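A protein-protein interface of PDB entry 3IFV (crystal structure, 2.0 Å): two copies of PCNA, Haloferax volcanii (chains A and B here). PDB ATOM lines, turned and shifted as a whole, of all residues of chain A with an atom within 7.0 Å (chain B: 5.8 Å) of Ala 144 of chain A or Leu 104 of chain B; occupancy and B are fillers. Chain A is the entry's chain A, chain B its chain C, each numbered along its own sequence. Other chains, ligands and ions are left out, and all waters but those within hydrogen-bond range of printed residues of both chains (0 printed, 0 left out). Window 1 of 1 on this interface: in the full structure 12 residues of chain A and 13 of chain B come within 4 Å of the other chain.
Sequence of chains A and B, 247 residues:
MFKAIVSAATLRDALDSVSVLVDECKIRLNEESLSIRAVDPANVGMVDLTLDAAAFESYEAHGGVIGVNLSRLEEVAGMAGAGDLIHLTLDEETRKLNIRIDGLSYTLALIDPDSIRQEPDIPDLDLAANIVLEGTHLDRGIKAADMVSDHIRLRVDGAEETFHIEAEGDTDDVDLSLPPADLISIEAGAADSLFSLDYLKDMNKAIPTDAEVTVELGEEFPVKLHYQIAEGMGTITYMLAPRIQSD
The backbone carbonyl oxygen (O) of Gly 103 of chain B lies within hydrogen-bond range of the backbone NH (N) of Ser 177 of chain A, at 3.0 Å.
N of Ser 105 of chain B lies within hydrogen-bond range of O of Asp 175 of chain A.
The guanidinium group (NH2) of Arg 140 of chain A is in hydrogen-bond range of the backbone carbonyl oxygen (O) of Ile 101 of chain B.
O of Met 79 of chain B lies within hydrogen-bond range of NH1 of Arg 140 of chain A.
The backbone NH (N) of Tyr 106 of chain B sits at hydrogen-bond distance from the backbone carbonyl oxygen (O) of Ile 99 of chain B, 2.9 Å away.
The backbone carbonyl oxygen (O) of Ile 165 of chain A is in hydrogen-bond range of the backbone NH (N) of Leu 176 of chain A (2.8 Å).
O of Ala 167 of chain A lies within hydrogen-bond range of N of Val 174 of chain A, 3.0 Å away.
Arg 140 of chain A touches Asp 102 of chain B (NH2 to CB, 3.7 Å).
NH2 of Arg 140 of chain A touches CB of Leu 104 of chain B (3.9 Å).
SD of Met 79 of chain B touches CE of Lys 143 of chain A, at 3.6 Å.
CE of Met 79 of chain B touches CB of Ala 144 of chain A (3.7 Å).
CD2 of Leu 104 of chain B touches CB of Ala 144 of chain A, at 3.6 Å.
Leu 104 of chain B touches Val 174 of chain A (CD1 to CG2, 3.6 Å).
CB of Val 174 of chain A touches CD1 of Tyr 106 of chain B (3.9 Å).
Asp 175 of chain A touches Gly 103 of chain B.
CA of Leu 104 of chain B touches O of Asp 175 of chain A, 3.7 Å away.
Leu 104 of chain B touches Leu 176 of chain A (CD1 to CB, 3.8 Å).
Of the printed residues of chain B, Ala 144 of chain A touches Met 79 and Leu 104.
Of the printed residues of chain A, Leu 104 of chain B touches Arg 140 (3.9 Å), Ala 144 (3.6 Å), Val 174 (3.6 Å), Asp 175 (3.7 Å) and Leu 176 (3.8 Å).
Of the printed residues of chain B, Asp 175 of chain A touches Gly 103, Leu 104 and Ser 105.
Printed residues of chain B within 4 Å of Lys 143 of chain A: Met 79 (3.6 Å).
Of the printed residues of chain A, Ile 101 of chain B touches Arg 140 (2.8 Å).
Of the printed residues of chain A, Tyr 106 of chain B touches Val 148 and Val 174.
Met 147 of chain A touches none of the printed residues of chain B.
Asp 146 of chain A touches none of the printed residues of chain B.
The nearest printed residue of chain A that does not touch Ile 101 of chain B is Leu 176 of chain A (5.8 Å).
Hydrophobic or aromatic side chains of chain B that line the printed part of chain A: Met 79, Ile 101, Leu 104 and Tyr 106.
Printed residues of chain A that touch a printed residue of chain B: Arg 140, Lys 143, Ala 144, Val 148, Val 174, Asp 175, Leu 176 and Ser 177.
Hydrophobic or aromatic side chains of chain A within 4 Å of the printed part of chain B: Ala 144, Val 148, Val 174 and Leu 176.
Among the printed residues, 17 pairs touch across the chains.
No position is printed for both chains.
Of the 17 pairs that touch across the chains among the printed residues, none has its exchanged pair printed and touching as well.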
ATOM      1  N   LEU A 138      19.698   4.805 -30.013  1.00  0.00           N
ATOM      2  CA  LEU A 138      20.877   5.541 -30.439  1.00  0.00           C
ATOM      3  C   LEU A 138      20.609   7.079 -30.629  1.00  0.00           C
ATOM      4  O   LEU A 138      21.456   7.923 -30.250  1.00  0.00           O
ATOM      5  CB  LEU A 138      21.479   4.870 -31.701  1.00  0.00           C
ATOM      6  CG  LEU A 138      22.670   5.489 -32.424  1.00  0.00           C
ATOM      7  CD1 LEU A 138      23.978   5.395 -31.586  1.00  0.00           C
ATOM      8  CD2 LEU A 138      22.917   4.755 -33.855  1.00  0.00           C
ATOM      9  N   ASP A 139      19.486   7.443 -31.223  1.00  0.00           N
ATOM     10  CA  ASP A 139      19.017   8.853 -31.168  1.00  0.00           C
ATOM     11  C   ASP A 139      19.092   9.453 -29.787  1.00  0.00           C
ATOM     12  O   ASP A 139      19.676  10.517 -29.493  1.00  0.00           O
ATOM     13  CB  ASP A 139      17.531   8.899 -31.428  1.00  0.00           C
ATOM     14  CG  ASP A 139      17.143   8.471 -32.826  1.00  0.00           C
ATOM     15  OD1 ASP A 139      18.013   8.017 -33.620  1.00  0.00           O
ATOM     16  OD2 ASP A 139      15.923   8.585 -33.120  1.00  0.00           O
ATOM     17  N   ARG A 140      18.362   8.759 -28.930  1.00  0.00           N
ATOM     18  CA  ARG A 140      18.265   9.092 -27.537  1.00  0.00           C
ATOM     19  C   ARG A 140      19.588   9.202 -26.793  1.00  0.00           C
ATOM     20  O   ARG A 140      19.767  10.122 -26.018  1.00  0.00           O
ATOM     21  CB  ARG A 140      17.363   8.060 -26.823  1.00  0.00           C
ATOM     22  CG  ARG A 140      17.206   8.269 -25.346  1.00  0.00           C
ATOM     23  CD  ARG A 140      15.807   7.691 -24.964  1.00  0.00           C
ATOM     24  NE  ARG A 140      15.617   7.442 -23.544  1.00  0.00           N
ATOM     25  CZ  ARG A 140      14.855   8.222 -22.792  1.00  0.00           C
ATOM     26  NH1 ARG A 140      14.261   9.281 -23.357  1.00  0.00           N
ATOM     27  NH2 ARG A 140      14.679   7.950 -21.506  1.00  0.00           N
ATOM     28  N   GLY A 141      20.465   8.223 -26.946  1.00  0.00           N
ATOM     29  CA  GLY A 141      21.774   8.304 -26.308  1.00  0.00           C
ATOM     30  C   GLY A 141      22.581   9.475 -26.808  1.00  0.00           C
ATOM     31  O   GLY A 141      23.253  10.139 -26.010  1.00  0.00           O
ATOM     32  N   ILE A 142      22.504   9.753 -28.112  1.00  0.00           N
ATOM     33  CA  ILE A 142      23.306  10.873 -28.688  1.00  0.00           C
ATOM     34  C   ILE A 142      22.798  12.232 -28.192  1.00  0.00           C
ATOM     35  O   ILE A 142      23.608  13.101 -27.890  1.00  0.00           O
ATOM     36  CB  ILE A 142      23.351  10.852 -30.251  1.00  0.00           C
ATOM     37  CG1 ILE A 142      24.088   9.603 -30.697  1.00  0.00           C
ATOM     38  CG2 ILE A 142      24.110  12.098 -30.848  1.00  0.00           C
ATOM     39  CD1 ILE A 142      23.943   9.311 -32.167  1.00  0.00           C
ATOM     40  N   LYS A 143      21.481  12.404 -28.144  1.00  0.00           N
ATOM     41  CA  LYS A 143      20.856  13.661 -27.682  1.00  0.00           C
ATOM     42  C   LYS A 143      21.244  13.921 -26.228  1.00  0.00           C
ATOM     43  O   LYS A 143      21.711  15.019 -25.905  1.00  0.00           O
ATOM     44  CB  LYS A 143      19.324  13.589 -27.878  1.00  0.00           C
ATOM     45  CG  LYS A 143      18.472  14.859 -27.529  1.00  0.00           C
ATOM     46  CD  LYS A 143      16.920  14.490 -27.422  1.00  0.00           C
ATOM     47  CE  LYS A 143      16.108  15.425 -26.469  1.00  0.00           C
ATOM     48  NZ  LYS A 143      16.011  16.888 -26.831  1.00  0.00           N
ATOM     49  N   ALA A 144      21.172  12.898 -25.374  1.00  0.00           N
ATOM     50  CA  ALA A 144      21.578  13.067 -24.003  1.00  0.00           C
ATOM     51  C   ALA A 144      23.075  13.343 -23.812  1.00  0.00           C
ATOM     52  O   ALA A 144      23.465  14.339 -23.150  1.00  0.00           O
ATOM     53  CB  ALA A 144      21.052  11.917 -23.080  1.00  0.00           C
ATOM     54  N   ALA A 145      23.922  12.532 -24.421  1.00  0.00           N
ATOM     55  CA  ALA A 145      25.375  12.820 -24.401  1.00  0.00           C
ATOM     56  C   ALA A 145      25.740  14.226 -24.810  1.00  0.00           C
ATOM     57  O   ALA A 145      26.674  14.811 -24.214  1.00  0.00           O
ATOM     58  CB  ALA A 145      26.110  11.866 -25.310  1.00  0.00           C
ATOM     59  N   ASP A 146      25.097  14.728 -25.879  1.00  0.00           N
ATOM     60  CA  ASP A 146      25.367  16.093 -26.434  1.00  0.00           C
ATOM     61  C   ASP A 146      25.191  17.266 -25.393  1.00  0.00           C
ATOM     62  O   ASP A 146      25.935  18.295 -25.443  1.00  0.00           O
ATOM     63  CB  ASP A 146      24.483  16.321 -27.670  1.00  0.00           C
ATOM     64  CG  ASP A 146      25.092  17.309 -28.705  1.00  0.00           C
ATOM     65  OD1 ASP A 146      26.240  17.694 -28.637  1.00  0.00           O
ATOM     66  OD2 ASP A 146      24.425  17.642 -29.681  1.00  0.00           O
ATOM     67  N   MET A 147      24.245  17.111 -24.464  1.00  0.00           N
ATOM     68  CA  MET A 147      24.040  18.103 -23.371  1.00  0.00           C
ATOM     69  C   MET A 147      25.312  18.277 -22.527  1.00  0.00           C
ATOM     70  O   MET A 147      25.512  19.310 -21.870  1.00  0.00           O
ATOM     71  CB  MET A 147      22.891  17.650 -22.422  1.00  0.00           C
ATOM     72  CG  MET A 147      21.539  17.531 -23.112  1.00  0.00           C
ATOM     73  SD  MET A 147      20.316  16.806 -21.986  1.00  0.00           S
ATOM     74  CE  MET A 147      20.538  17.877 -20.570  1.00  0.00           C
ATOM     75  N   VAL A 148      26.192  17.272 -22.496  1.00  0.00           N
ATOM     76  CA  VAL A 148      27.350  17.401 -21.604  1.00  0.00           C
ATOM     77  C   VAL A 148      28.689  17.412 -22.281  1.00  0.00           C
ATOM     78  O   VAL A 148      29.634  17.960 -21.728  1.00  0.00           O
ATOM     79  CB  VAL A 148      27.438  16.309 -20.453  1.00  0.00           C
ATOM     80  CG1 VAL A 148      26.084  16.095 -19.771  1.00  0.00           C
ATOM     81  CG2 VAL A 148      28.048  14.997 -20.987  1.00  0.00           C
ATOM     82  N   SER A 149      28.836  16.775 -23.438  1.00  0.00           N
ATOM     83  CA  SER A 149      30.193  16.767 -24.087  1.00  0.00           C
ATOM     84  C   SER A 149      30.078  16.776 -25.621  1.00  0.00           C
ATOM     85  O   SER A 149      28.997  16.617 -26.153  1.00  0.00           O
ATOM     86  CB  SER A 149      30.939  15.508 -23.606  1.00  0.00           C
ATOM     87  OG  SER A 149      32.226  15.367 -24.137  1.00  0.00           O
ATOM     88  N   ILE A 152      31.492  11.207 -27.292  1.00  0.00           N
ATOM     89  CA  ILE A 152      30.483  10.167 -26.897  1.00  0.00           C
ATOM     90  C   ILE A 152      31.235   8.837 -26.823  1.00  0.00           C
ATOM     91  O   ILE A 152      32.050   8.540 -27.716  1.00  0.00           O
ATOM     92  CB  ILE A 152      29.267  10.085 -27.888  1.00  0.00           C
ATOM     93  CG1 ILE A 152      28.099   9.275 -27.320  1.00  0.00           C
ATOM     94  CG2 ILE A 152      29.646   9.517 -29.232  1.00  0.00           C
ATOM     95  CD1 ILE A 152      26.759   9.501 -28.055  1.00  0.00           C
ATOM     96  N   ILE A 165      25.714   3.931 -23.807  1.00  0.00           N
ATOM     97  CA  ILE A 165      26.015   5.136 -24.578  1.00  0.00           C
ATOM     98  C   ILE A 165      26.190   6.211 -23.540  1.00  0.00           C
ATOM     99  O   ILE A 165      25.263   6.560 -22.846  1.00  0.00           O
ATOM    100  CB  ILE A 165      24.837   5.510 -25.586  1.00  0.00           C
ATOM    101  CG1 ILE A 165      24.522   4.285 -26.460  1.00  0.00           C
ATOM    102  CG2 ILE A 165      25.213   6.773 -26.438  1.00  0.00           C
ATOM    103  CD1 ILE A 165      23.232   4.493 -27.411  1.00  0.00           C
ATOM    104  N   ALA A 167      28.489   9.769 -21.747  1.00  0.00           N
ATOM    105  CA  ALA A 167      29.366  10.906 -21.837  1.00  0.00           C
ATOM    106  C   ALA A 167      29.728  11.499 -20.505  1.00  0.00           C
ATOM    107  O   ALA A 167      28.944  11.484 -19.584  1.00  0.00           O
ATOM    108  CB  ALA A 167      28.772  11.990 -22.751  1.00  0.00           C
ATOM    109  N   VAL A 174      26.330  11.414 -18.145  1.00  0.00           N
ATOM    110  CA  VAL A 174      25.098  10.746 -18.568  1.00  0.00           C
ATOM    111  C   VAL A 174      25.481   9.337 -19.066  1.00  0.00           C
ATOM    112  O   VAL A 174      26.583   9.149 -19.533  1.00  0.00           O
ATOM    113  CB  VAL A 174      24.386  11.594 -19.633  1.00  0.00           C
ATOM    114  CG1 VAL A 174      25.227  11.642 -20.903  1.00  0.00           C
ATOM    115  CG2 VAL A 174      22.948  11.059 -19.881  1.00  0.00           C
ATOM    116  N   ASP A 175      24.562   8.377 -18.960  1.00  0.00           N
ATOM    117  CA  ASP A 175      24.804   7.004 -19.293  1.00  0.00           C
ATOM    118  C   ASP A 175      23.428   6.449 -19.655  1.00  0.00           C
ATOM    119  O   ASP A 175      22.533   6.368 -18.796  1.00  0.00           O
ATOM    120  CB  ASP A 175      25.492   6.282 -18.092  1.00  0.00           C
ATOM    121  CG  ASP A 175      25.457   4.757 -18.209  1.00  0.00           C
ATOM    122  OD1 ASP A 175      25.211   4.278 -19.333  1.00  0.00           O
ATOM    123  OD2 ASP A 175      25.642   4.050 -17.169  1.00  0.00           O
ATOM    124  N   LEU A 176      23.180   6.237 -20.959  1.00  0.00           N
ATOM    125  CA  LEU A 176      22.031   5.422 -21.367  1.00  0.00           C
ATOM    126  C   LEU A 176      22.421   3.947 -21.311  1.00  0.00           C
ATOM    127  O   LEU A 176      23.263   3.501 -22.109  1.00  0.00           O
ATOM    128  CB  LEU A 176      21.658   5.753 -22.771  1.00  0.00           C
ATOM    129  CG  LEU A 176      20.614   4.901 -23.462  1.00  0.00           C
ATOM    130  CD1 LEU A 176      19.386   4.908 -22.596  1.00  0.00           C
ATOM    131  CD2 LEU A 176      20.402   5.583 -24.888  1.00  0.00           C
ATOM    132  N   SER A 177      21.857   3.222 -20.337  1.00  0.00           N
ATOM    133  CA  SER A 177      22.237   1.841 -20.084  1.00  0.00           C
ATOM    134  C   SER A 177      21.181   0.918 -20.721  1.00  0.00           C
ATOM    135  O   SER A 177      19.987   1.018 -20.433  1.00  0.00           O
ATOM    136  CB  SER A 177      22.366   1.635 -18.579  1.00  0.00           C
ATOM    137  OG  SER A 177      22.580   0.275 -18.283  1.00  0.00           O
ATOM    138  N   LEU A 197      31.193  13.103 -31.195  1.00  0.00           N
ATOM    139  CA  LEU A 197      29.754  12.993 -31.123  1.00  0.00           C
ATOM    140  C   LEU A 197      29.151  13.676 -32.364  1.00  0.00           C
ATOM    141  O   LEU A 197      28.126  13.213 -32.879  1.00  0.00           O
ATOM    142  CB  LEU A 197      29.217  13.636 -29.813  1.00  0.00           C
ATOM    143  CG  LEU A 197      27.712  13.636 -29.570  1.00  0.00           C
ATOM    144  CD1 LEU A 197      27.387  13.777 -28.105  1.00  0.00           C
ATOM    145  CD2 LEU A 197      26.900  14.656 -30.355  1.00  0.00           C
ATOM    146  N   MET B  79      14.212  15.272 -22.012  1.00  0.00           N
ATOM    147  CA  MET B  79      14.354  13.963 -22.670  1.00  0.00           C
ATOM    148  C   MET B  79      13.187  13.012 -22.399  1.00  0.00           C
ATOM    149  O   MET B  79      13.100  12.011 -23.049  1.00  0.00           O
ATOM    150  CB  MET B  79      15.590  13.233 -22.188  1.00  0.00           C
ATOM    151  CG  MET B  79      16.856  14.056 -22.059  1.00  0.00           C
ATOM    152  SD  MET B  79      17.786  13.987 -23.577  1.00  0.00           S
ATOM    153  CE  MET B  79      17.526  12.328 -24.210  1.00  0.00           C
ATOM    154  N   ILE B  99      19.153  11.812 -11.945  1.00  0.00           N
ATOM    155  CA  ILE B  99      17.887  11.856 -12.611  1.00  0.00           C
ATOM    156  C   ILE B  99      17.905  10.641 -13.535  1.00  0.00           C
ATOM    157  O   ILE B  99      18.823  10.446 -14.258  1.00  0.00           O
ATOM    158  CB  ILE B  99      17.794  13.127 -13.452  1.00  0.00           C
ATOM    159  CG1 ILE B  99      17.986  14.365 -12.548  1.00  0.00           C
ATOM    160  CG2 ILE B  99      16.474  13.186 -14.251  1.00  0.00           C
ATOM    161  CD1 ILE B  99      18.546  15.565 -13.274  1.00  0.00           C
ATOM    162  N   ARG B 100      16.886   9.803 -13.470  1.00  0.00           N
ATOM    163  CA  ARG B 100      16.833   8.614 -14.307  1.00  0.00           C
ATOM    164  C   ARG B 100      15.503   8.592 -15.064  1.00  0.00           C
ATOM    165  O   ARG B 100      14.480   8.867 -14.477  1.00  0.00           O
ATOM    166  CB  ARG B 100      16.971   7.372 -13.400  1.00  0.00           C
ATOM    167  CG  ARG B 100      17.001   6.033 -14.199  1.00  0.00           C
ATOM    168  CD  ARG B 100      17.060   4.895 -13.212  1.00  0.00           C
ATOM    169  NE  ARG B 100      15.765   4.226 -13.093  1.00  0.00           N
ATOM    170  CZ  ARG B 100      15.029   4.142 -11.989  1.00  0.00           C
ATOM    171  NH1 ARG B 100      15.423   4.716 -10.866  1.00  0.00           N
ATOM    172  NH2 ARG B 100      13.879   3.490 -12.020  1.00  0.00           N
ATOM    173  N   ILE B 101      15.522   8.337 -16.369  1.00  0.00           N
ATOM    174  CA  ILE B 101      14.307   8.287 -17.166  1.00  0.00           C
ATOM    175  C   ILE B 101      14.535   7.042 -18.017  1.00  0.00           C
ATOM    176  O   ILE B 101      15.372   7.056 -18.944  1.00  0.00           O
ATOM    177  CB  ILE B 101      14.175   9.470 -18.151  1.00  0.00           C
ATOM    178  CG1 ILE B 101      14.265  10.816 -17.473  1.00  0.00           C
ATOM    179  CG2 ILE B 101      12.917   9.373 -18.911  1.00  0.00           C
ATOM    180  CD1 ILE B 101      14.498  12.001 -18.512  1.00  0.00           C
ATOM    181  N   ASP B 102      13.823   5.974 -17.667  1.00  0.00           N
ATOM    182  CA  ASP B 102      14.019   4.676 -18.277  1.00  0.00           C
ATOM    183  C   ASP B 102      15.425   4.170 -18.014  1.00  0.00           C
ATOM    184  O   ASP B 102      15.916   4.134 -16.871  1.00  0.00           O
ATOM    185  CB  ASP B 102      13.808   4.781 -19.755  1.00  0.00           C
ATOM    186  CG  ASP B 102      12.426   4.329 -20.158  1.00  0.00           C
ATOM    187  OD1 ASP B 102      11.602   4.139 -19.217  1.00  0.00           O
ATOM    188  OD2 ASP B 102      12.165   4.154 -21.382  1.00  0.00           O
ATOM    189  N   GLY B 103      16.113   3.810 -19.069  1.00  0.00           N
ATOM    190  CA  GLY B 103      17.460   3.377 -18.839  1.00  0.00           C
ATOM    191  C   GLY B 103      18.454   4.532 -18.802  1.00  0.00           C
ATOM    192  O   GLY B 103      19.630   4.265 -18.627  1.00  0.00           O
ATOM    193  N   LEU B 104      18.015   5.776 -19.047  1.00  0.00           N
ATOM    194  CA  LEU B 104      18.914   6.985 -19.074  1.00  0.00           C
ATOM    195  C   LEU B 104      19.222   7.612 -17.707  1.00  0.00           C
ATOM    196  O   LEU B 104      18.328   8.102 -17.050  1.00  0.00           O
ATOM    197  CB  LEU B 104      18.302   8.101 -19.973  1.00  0.00           C
ATOM    198  CG  LEU B 104      19.085   9.372 -20.348  1.00  0.00           C
ATOM    199  CD1 LEU B 104      20.290   8.913 -21.156  1.00  0.00           C
ATOM    200  CD2 LEU B 104      18.309  10.396 -21.254  1.00  0.00           C
ATOM    201  N   SER B 105      20.487   7.663 -17.295  1.00  0.00           N
ATOM    202  CA  SER B 105      20.823   8.126 -15.932  1.00  0.00           C
ATOM    203  C   SER B 105      21.775   9.286 -16.070  1.00  0.00           C
ATOM    204  O   SER B 105      22.861   9.091 -16.568  1.00  0.00           O
ATOM    205  CB  SER B 105      21.591   7.073 -15.110  1.00  0.00           C
ATOM    206  OG  SER B 105      20.797   5.978 -14.745  1.00  0.00           O
ATOM    207  N   TYR B 106      21.380  10.454 -15.545  1.00  0.00           N
ATOM    208  CA  TYR B 106      22.142  11.680 -15.660  1.00  0.00           C
ATOM    209  C   TYR B 106      22.526  12.107 -14.275  1.00  0.00           C
ATOM    210  O   TYR B 106      21.660  12.173 -13.388  1.00  0.00           O
ATOM    211  CB  TYR B 106      21.225  12.739 -16.344  1.00  0.00           C
ATOM    212  CG  TYR B 106      21.915  14.013 -16.638  1.00  0.00           C
ATOM    213  CD1 TYR B 106      22.286  14.347 -17.938  1.00  0.00           C
ATOM    214  CD2 TYR B 106      22.206  14.900 -15.637  1.00  0.00           C
ATOM    215  CE1 TYR B 106      22.980  15.534 -18.212  1.00  0.00           C
ATOM    216  CE2 TYR B 106      22.902  16.110 -15.898  1.00  0.00           C
ATOM    217  CZ  TYR B 106      23.269  16.418 -17.194  1.00  0.00           C
ATOM    218  OH  TYR B 106      23.946  17.604 -17.455  1.00  0.00           O
